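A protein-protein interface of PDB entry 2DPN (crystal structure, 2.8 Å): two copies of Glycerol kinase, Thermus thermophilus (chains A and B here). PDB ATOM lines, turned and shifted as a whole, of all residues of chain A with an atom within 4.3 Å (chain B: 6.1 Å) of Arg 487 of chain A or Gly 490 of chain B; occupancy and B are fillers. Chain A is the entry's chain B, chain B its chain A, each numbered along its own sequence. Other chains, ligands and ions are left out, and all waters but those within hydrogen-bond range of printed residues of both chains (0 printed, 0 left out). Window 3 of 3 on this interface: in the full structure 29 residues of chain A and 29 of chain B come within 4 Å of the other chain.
NH1 of Arg 487 of chain B lies within hydrogen-bond range of O of Arg 487 of chain A, at 2.7 Å.
NH2 of Arg 487 of chain B is in hydrogen-bond range of O of Lys 489 of chain A.
The guanidinium group (NH1) of Arg 487 of chain A sits at hydrogen-bond distance from the backbone carbonyl oxygen (O) of Lys 489 of chain B (2.6 Å).
O of Gly 490 of chain B lies within hydrogen-bond range of NH2 of Arg 487 of chain A.
The side-chain carboxylate (OD2) of Asp 353 of chain B is in hydrogen-bond range of the backbone NH (N) of Gly 490 of chain B.
The backbone carbonyl oxygen (O) of Tyr 355 of chain B sits at hydrogen-bond distance from the backbone NH (N) of Trp 491 of chain B.
The backbone carbonyl oxygen (O) of Ala 488 of chain B sits at hydrogen-bond distance from the backbone NH (N) of Arg 357 of chain B.
NZ of Lys 489 of chain B is in salt-bridge range of OE1 of Glu 486 of chain B (2.9 Å).
The side-chain carboxylate (OE1) of Glu 483 of chain A lies within salt-bridge range of the guanidinium group (NE) of Arg 487 of chain A (3.3 Å).
The side-chain carboxylate (OE1) of Glu 486 of chain A is in salt-bridge range of the side-chain amino group (NZ) of Lys 489 of chain A, at 3.0 Å.
Among the printed residues, merely in contact across the chains: Ala 484 of chain A with Trp 491 of chain B, Thr 359 of chain A with Leu 361 of chain B, Arg 487 of chain A with Trp 491 of chain B, Arg 487 of chain A with Ala 488 of chain B, Ala 488 of chain A with Arg 487 of chain B and Arg 487 of chain A with Leu 361 of chain B.
Of chain A, only Arg 487 (2.6 Å) comes within 4 Å of Gly 490 of chain B.
Of the printed residues of chain A, Ala 488 of chain B touches Arg 487 (3.9 Å).
Of the printed residues of chain A, Leu 361 of chain B touches Thr 359 (3.7 Å) and Arg 487 (3.96 Å).
Printed residues of chain B within 4 Å of Ala 488 of chain A: Arg 487 (3.9 Å).
Printed residues of chain A within 4 Å of Trp 491 of chain B: Ala 484 (3.6 Å) and Arg 487 (3.8 Å).
Printed residues of chain B within 4 Å of Lys 489 of chain A: Arg 487 (2.9 Å).
Ala 492 of chain B touches none of the printed residues of chain A.
Glu 494 of chain B touches none of the printed residues of chain A.
The nearest residue of chain B that does not touch Arg 487 of chain A is Glu 486 of chain B (4.5 Å).
The nearest printed residue of chain A that does not touch Gly 490 of chain B is Glu 483 of chain A (6.2 Å).
Hydrophobic or aromatic side chains of chain A within 4 Å of the printed part of chain B: Ala 484.
Along chain A the printed residues that touch a printed residue of chain B span positions 359 to 489.
Hydrophobic or aromatic side chains of chain B within 4 Å of the printed part of chain A: Leu 361 and Trp 491.
Among the printed residues, no Asp or Glu carboxylate lies within 4 Å of a Lys or Arg side-chain nitrogen of the other chain.
Arg 487 of chain B touches its own counterpart, Arg 487 of chain A.
Arg 487 of chain A touches Ala 488 of chain B, and with the chains exchanged Ala 488 of chain A touches Arg 487 of chain B.
Arg 487 of chain A touches Lys 489 of chain B, and with the chains exchanged Lys 489 of chain A touches Arg 487 of chain B.
Positions printed for both chains: 486, 487, 488 and 489.
Of the 10 pairs that touch across the chains among the printed residues, 5 have their exchanged pair printed and touching as well.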
ATOM      1  N   THR A 359     -17.924  -9.898  33.904  1.00  0.00           N
ATOM      2  CA  THR A 359     -18.475 -10.282  32.613  1.00  0.00           C
ATOM      3  C   THR A 359     -18.678  -9.110  31.638  1.00  0.00           C
ATOM      4  O   THR A 359     -19.161  -8.043  32.017  1.00  0.00           O
ATOM      5  CB  THR A 359     -19.840 -10.977  32.830  1.00  0.00           C
ATOM      6  OG1 THR A 359     -19.673 -12.074  33.730  1.00  0.00           O
ATOM      7  CG2 THR A 359     -20.425 -11.463  31.522  1.00  0.00           C
ATOM      8  N   GLU A 483     -30.278  -8.253  32.311  1.00  0.00           N
ATOM      9  CA  GLU A 483     -30.117  -9.490  31.581  1.00  0.00           C
ATOM     10  C   GLU A 483     -28.627  -9.796  31.641  1.00  0.00           C
ATOM     11  O   GLU A 483     -28.214 -10.945  31.753  1.00  0.00           O
ATOM     12  CB  GLU A 483     -30.576  -9.340  30.139  1.00  0.00           C
ATOM     13  CG  GLU A 483     -30.512 -10.645  29.364  1.00  0.00           C
ATOM     14  CD  GLU A 483     -30.846 -11.848  30.242  1.00  0.00           C
ATOM     15  OE1 GLU A 483     -29.956 -12.718  30.441  1.00  0.00           O
ATOM     16  OE2 GLU A 483     -31.998 -11.916  30.738  1.00  0.00           O
ATOM     17  N   ALA A 484     -27.821  -8.747  31.590  1.00  0.00           N
ATOM     18  CA  ALA A 484     -26.381  -8.901  31.661  1.00  0.00           C
ATOM     19  C   ALA A 484     -25.980  -9.555  32.994  1.00  0.00           C
ATOM     20  O   ALA A 484     -25.148 -10.468  33.029  1.00  0.00           O
ATOM     21  CB  ALA A 484     -25.717  -7.545  31.513  1.00  0.00           C
ATOM     22  N   VAL A 485     -26.580  -9.092  34.086  1.00  0.00           N
ATOM     23  CA  VAL A 485     -26.274  -9.632  35.404  1.00  0.00           C
ATOM     24  C   VAL A 485     -26.650 -11.103  35.515  1.00  0.00           C
ATOM     25  O   VAL A 485     -25.983 -11.871  36.206  1.00  0.00           O
ATOM     26  CB  VAL A 485     -26.993  -8.839  36.511  1.00  0.00           C
ATOM     27  CG1 VAL A 485     -26.700  -9.461  37.880  1.00  0.00           C
ATOM     28  CG2 VAL A 485     -26.533  -7.391  36.481  1.00  0.00           C
ATOM     29  N   GLU A 486     -27.716 -11.499  34.832  1.00  0.00           N
ATOM     30  CA  GLU A 486     -28.143 -12.898  34.851  1.00  0.00           C
ATOM     31  C   GLU A 486     -27.102 -13.818  34.204  1.00  0.00           C
ATOM     32  O   GLU A 486     -27.114 -15.023  34.431  1.00  0.00           O
ATOM     33  CB  GLU A 486     -29.476 -13.076  34.112  1.00  0.00           C
ATOM     34  CG  GLU A 486     -30.695 -12.505  34.814  1.00  0.00           C
ATOM     35  CD  GLU A 486     -31.010 -13.202  36.132  1.00  0.00           C
ATOM     36  OE1 GLU A 486     -30.442 -12.814  37.180  1.00  0.00           O
ATOM     37  OE2 GLU A 486     -31.828 -14.149  36.116  1.00  0.00           O
ATOM     38  N   ARG A 487     -26.209 -13.267  33.388  1.00  0.00           N
ATOM     39  CA  ARG A 487     -25.202 -14.105  32.746  1.00  0.00           C
ATOM     40  C   ARG A 487     -23.838 -14.092  33.425  1.00  0.00           C
ATOM     41  O   ARG A 487     -22.905 -14.772  32.991  1.00  0.00           O
ATOM     42  CB  ARG A 487     -25.066 -13.736  31.270  1.00  0.00           C
ATOM     43  CG  ARG A 487     -26.325 -14.019  30.515  1.00  0.00           C
ATOM     44  CD  ARG A 487     -26.174 -13.842  29.041  1.00  0.00           C
ATOM     45  NE  ARG A 487     -27.491 -13.671  28.438  1.00  0.00           N
ATOM     46  CZ  ARG A 487     -27.762 -13.885  27.157  1.00  0.00           C
ATOM     47  NH1 ARG A 487     -26.801 -14.280  26.325  1.00  0.00           N
ATOM     48  NH2 ARG A 487     -29.003 -13.718  26.718  1.00  0.00           N
ATOM     49  N   ALA A 488     -23.717 -13.321  34.492  1.00  0.00           N
ATOM     50  CA  ALA A 488     -22.469 -13.282  35.219  1.00  0.00           C
ATOM     51  C   ALA A 488     -22.624 -14.228  36.409  1.00  0.00           C
ATOM     52  O   ALA A 488     -21.654 -14.818  36.889  1.00  0.00           O
ATOM     53  CB  ALA A 488     -22.189 -11.872  35.691  1.00  0.00           C
ATOM     54  N   LYS A 489     -23.866 -14.387  36.859  1.00  0.00           N
ATOM     55  CA  LYS A 489     -24.153 -15.232  38.009  1.00  0.00           C
ATOM     56  C   LYS A 489     -23.763 -16.692  37.893  1.00  0.00           C
ATOM     57  O   LYS A 489     -23.938 -17.319  36.859  1.00  0.00           O
ATOM     58  CB  LYS A 489     -25.637 -15.129  38.394  1.00  0.00           C
ATOM     59  CG  LYS A 489     -25.971 -13.824  39.071  1.00  0.00           C
ATOM     60  CD  LYS A 489     -27.184 -13.916  39.972  1.00  0.00           C
ATOM     61  CE  LYS A 489     -28.468 -13.842  39.170  1.00  0.00           C
ATOM     62  NZ  LYS A 489     -29.652 -13.486  40.018  1.00  0.00           N
ATOM     63  N   ASP B 353     -26.354 -19.150  15.564  1.00  0.00           N
ATOM     64  CA  ASP B 353     -27.168 -18.253  16.364  1.00  0.00           C
ATOM     65  C   ASP B 353     -26.796 -16.800  16.045  1.00  0.00           C
ATOM     66  O   ASP B 353     -25.828 -16.259  16.581  1.00  0.00           O
ATOM     67  CB  ASP B 353     -26.953 -18.557  17.852  1.00  0.00           C
ATOM     68  CG  ASP B 353     -27.625 -17.548  18.766  1.00  0.00           C
ATOM     69  OD1 ASP B 353     -28.552 -16.823  18.317  1.00  0.00           O
ATOM     70  OD2 ASP B 353     -27.228 -17.493  19.951  1.00  0.00           O
ATOM     71  N   TYR B 355     -27.953 -14.241  17.003  1.00  0.00           N
ATOM     72  CA  TYR B 355     -28.084 -13.417  18.182  1.00  0.00           C
ATOM     73  C   TYR B 355     -26.965 -13.360  19.181  1.00  0.00           C
ATOM     74  O   TYR B 355     -26.887 -12.396  19.952  1.00  0.00           O
ATOM     75  CB  TYR B 355     -29.394 -13.791  18.866  1.00  0.00           C
ATOM     76  CG  TYR B 355     -30.563 -13.506  17.962  1.00  0.00           C
ATOM     77  CD1 TYR B 355     -30.983 -12.197  17.765  1.00  0.00           C
ATOM     78  CD2 TYR B 355     -31.175 -14.522  17.224  1.00  0.00           C
ATOM     79  CE1 TYR B 355     -31.973 -11.896  16.861  1.00  0.00           C
ATOM     80  CE2 TYR B 355     -32.171 -14.229  16.308  1.00  0.00           C
ATOM     81  CZ  TYR B 355     -32.559 -12.905  16.134  1.00  0.00           C
ATOM     82  OH  TYR B 355     -33.529 -12.549  15.234  1.00  0.00           O
ATOM     83  N   ALA B 356     -26.094 -14.366  19.168  1.00  0.00           N
ATOM     84  CA  ALA B 356     -24.974 -14.408  20.106  1.00  0.00           C
ATOM     85  C   ALA B 356     -24.029 -13.224  19.894  1.00  0.00           C
ATOM     86  O   ALA B 356     -23.990 -12.648  18.801  1.00  0.00           O
ATOM     87  CB  ALA B 356     -24.215 -15.726  19.956  1.00  0.00           C
ATOM     88  N   ARG B 357     -23.287 -12.852  20.943  1.00  0.00           N
ATOM     89  CA  ARG B 357     -22.329 -11.748  20.863  1.00  0.00           C
ATOM     90  C   ARG B 357     -21.004 -12.029  21.588  1.00  0.00           C
ATOM     91  O   ARG B 357     -20.879 -13.013  22.319  1.00  0.00           O
ATOM     92  CB  ARG B 357     -22.965 -10.466  21.398  1.00  0.00           C
ATOM     93  CG  ARG B 357     -24.025  -9.875  20.467  1.00  0.00           C
ATOM     94  CD  ARG B 357     -23.406  -9.204  19.229  1.00  0.00           C
ATOM     95  NE  ARG B 357     -24.418  -8.628  18.342  1.00  0.00           N
ATOM     96  CZ  ARG B 357     -25.216  -9.341  17.547  1.00  0.00           C
ATOM     97  NH1 ARG B 357     -25.124 -10.665  17.511  1.00  0.00           N
ATOM     98  NH2 ARG B 357     -26.125  -8.728  16.802  1.00  0.00           N
ATOM     99  N   LEU B 361     -15.913 -14.073  30.039  1.00  0.00           N
ATOM    100  CA  LEU B 361     -16.382 -14.644  31.291  1.00  0.00           C
ATOM    101  C   LEU B 361     -15.264 -15.004  32.249  1.00  0.00           C
ATOM    102  O   LEU B 361     -14.192 -15.420  31.827  1.00  0.00           O
ATOM    103  CB  LEU B 361     -17.190 -15.897  31.001  1.00  0.00           C
ATOM    104  CG  LEU B 361     -18.414 -15.663  30.127  1.00  0.00           C
ATOM    105  CD1 LEU B 361     -18.857 -16.973  29.517  1.00  0.00           C
ATOM    106  CD2 LEU B 361     -19.518 -15.051  30.962  1.00  0.00           C
ATOM    107  N   GLU B 486     -22.891 -20.869  26.033  1.00  0.00           N
ATOM    108  CA  GLU B 486     -24.269 -20.690  26.467  1.00  0.00           C
ATOM    109  C   GLU B 486     -24.489 -19.261  26.923  1.00  0.00           C
ATOM    110  O   GLU B 486     -25.438 -18.610  26.496  1.00  0.00           O
ATOM    111  CB  GLU B 486     -24.600 -21.647  27.616  1.00  0.00           C
ATOM    112  CG  GLU B 486     -24.600 -23.094  27.208  1.00  0.00           C
ATOM    113  CD  GLU B 486     -25.566 -23.364  26.068  1.00  0.00           C
ATOM    114  OE1 GLU B 486     -25.295 -24.274  25.254  1.00  0.00           O
ATOM    115  OE2 GLU B 486     -26.602 -22.673  25.983  1.00  0.00           O
ATOM    116  N   ARG B 487     -23.607 -18.770  27.786  1.00  0.00           N
ATOM    117  CA  ARG B 487     -23.733 -17.413  28.289  1.00  0.00           C
ATOM    118  C   ARG B 487     -23.558 -16.370  27.199  1.00  0.00           C
ATOM    119  O   ARG B 487     -23.855 -15.190  27.403  1.00  0.00           O
ATOM    120  CB  ARG B 487     -22.743 -17.173  29.437  1.00  0.00           C
ATOM    121  CG  ARG B 487     -23.248 -17.677  30.785  1.00  0.00           C
ATOM    122  CD  ARG B 487     -22.165 -18.414  31.556  1.00  0.00           C
ATOM    123  NE  ARG B 487     -22.679 -19.138  32.725  1.00  0.00           N
ATOM    124  CZ  ARG B 487     -23.060 -18.573  33.870  1.00  0.00           C
ATOM    125  NH1 ARG B 487     -23.003 -17.255  34.036  1.00  0.00           N
ATOM    126  NH2 ARG B 487     -23.484 -19.340  34.861  1.00  0.00           N
ATOM    127  N   ALA B 488     -23.104 -16.805  26.031  1.00  0.00           N
ATOM    128  CA  ALA B 488     -22.907 -15.885  24.917  1.00  0.00           C
ATOM    129  C   ALA B 488     -24.096 -15.913  23.970  1.00  0.00           C
ATOM    130  O   ALA B 488     -24.433 -14.894  23.348  1.00  0.00           O
ATOM    131  CB  ALA B 488     -21.643 -16.238  24.167  1.00  0.00           C
ATOM    132  N   LYS B 489     -24.737 -17.074  23.873  1.00  0.00           N
ATOM    133  CA  LYS B 489     -25.877 -17.224  22.986  1.00  0.00           C
ATOM    134  C   LYS B 489     -27.014 -16.235  23.213  1.00  0.00           C
ATOM    135  O   LYS B 489     -27.278 -15.806  24.329  1.00  0.00           O
ATOM    136  CB  LYS B 489     -26.410 -18.657  23.036  1.00  0.00           C
ATOM    137  CG  LYS B 489     -25.642 -19.580  22.121  1.00  0.00           C
ATOM    138  CD  LYS B 489     -26.296 -20.936  21.920  1.00  0.00           C
ATOM    139  CE  LYS B 489     -26.092 -21.854  23.116  1.00  0.00           C
ATOM    140  NZ  LYS B 489     -26.169 -23.297  22.705  1.00  0.00           N
ATOM    141  N   GLY B 490     -27.654 -15.868  22.107  1.00  0.00           N
ATOM    142  CA  GLY B 490     -28.775 -14.952  22.113  1.00  0.00           C
ATOM    143  C   GLY B 490     -28.688 -13.761  23.033  1.00  0.00           C
ATOM    144  O   GLY B 490     -29.304 -13.750  24.092  1.00  0.00           O
ATOM    145  N   TRP B 491     -27.921 -12.755  22.635  1.00  0.00           N
ATOM    146  CA  TRP B 491     -27.799 -11.553  23.423  1.00  0.00           C
ATOM    147  C   TRP B 491     -28.570 -10.428  22.732  1.00  0.00           C
ATOM    148  O   TRP B 491     -29.078  -9.524  23.379  1.00  0.00           O
ATOM    149  CB  TRP B 491     -26.337 -11.169  23.590  1.00  0.00           C
ATOM    150  CG  TRP B 491     -26.187  -9.831  24.223  1.00  0.00           C
ATOM    151  CD1 TRP B 491     -25.925  -8.648  23.590  1.00  0.00           C
ATOM    152  CD2 TRP B 491     -26.383  -9.512  25.606  1.00  0.00           C
ATOM    153  NE1 TRP B 491     -25.947  -7.612  24.496  1.00  0.00           N
ATOM    154  CE2 TRP B 491     -26.226  -8.115  25.740  1.00  0.00           C
ATOM    155  CE3 TRP B 491     -26.682 -10.272  26.744  1.00  0.00           C
ATOM    156  CZ2 TRP B 491     -26.356  -7.458  26.971  1.00  0.00           C
ATOM    157  CZ3 TRP B 491     -26.814  -9.623  27.968  1.00  0.00           C
ATOM    158  CH2 TRP B 491     -26.650  -8.226  28.070  1.00  0.00           C
ATOM    159  N   ALA B 492     -28.665 -10.495  21.411  1.00  0.00           N
ATOM    160  CA  ALA B 492     -29.379  -9.480  20.654  1.00  0.00           C
ATOM    161  C   ALA B 492     -30.862  -9.811  20.609  1.00  0.00           C
ATOM    162  O   ALA B 492     -31.254 -10.942  20.865  1.00  0.00           O
ATOM    163  CB  ALA B 492     -28.816  -9.394  19.260  1.00  0.00           C
ATOM    164  N   GLU B 494     -34.551 -10.619  19.097  1.00  0.00           N
ATOM    165  CA  GLU B 494     -35.091 -11.342  17.947  1.00  0.00           C
ATOM    166  C   GLU B 494     -36.385 -10.717  17.409  1.00  0.00           C
ATOM    167  O   GLU B 494     -37.296 -11.476  17.010  1.00  0.00           O
ATOM    168  CB  GLU B 494     -35.334 -12.812  18.321  1.00  0.00           C
ATOM    169  CG  GLU B 494     -34.152 -13.478  19.035  1.00  0.00           C
ATOM    170  CD  GLU B 494     -34.265 -15.001  19.115  1.00  0.00           C
ATOM    171  OE1 GLU B 494     -33.426 -15.630  19.804  1.00  0.00           O
ATOM    172  OE2 GLU B 494     -35.183 -15.565  18.485  1.00  0.00           O
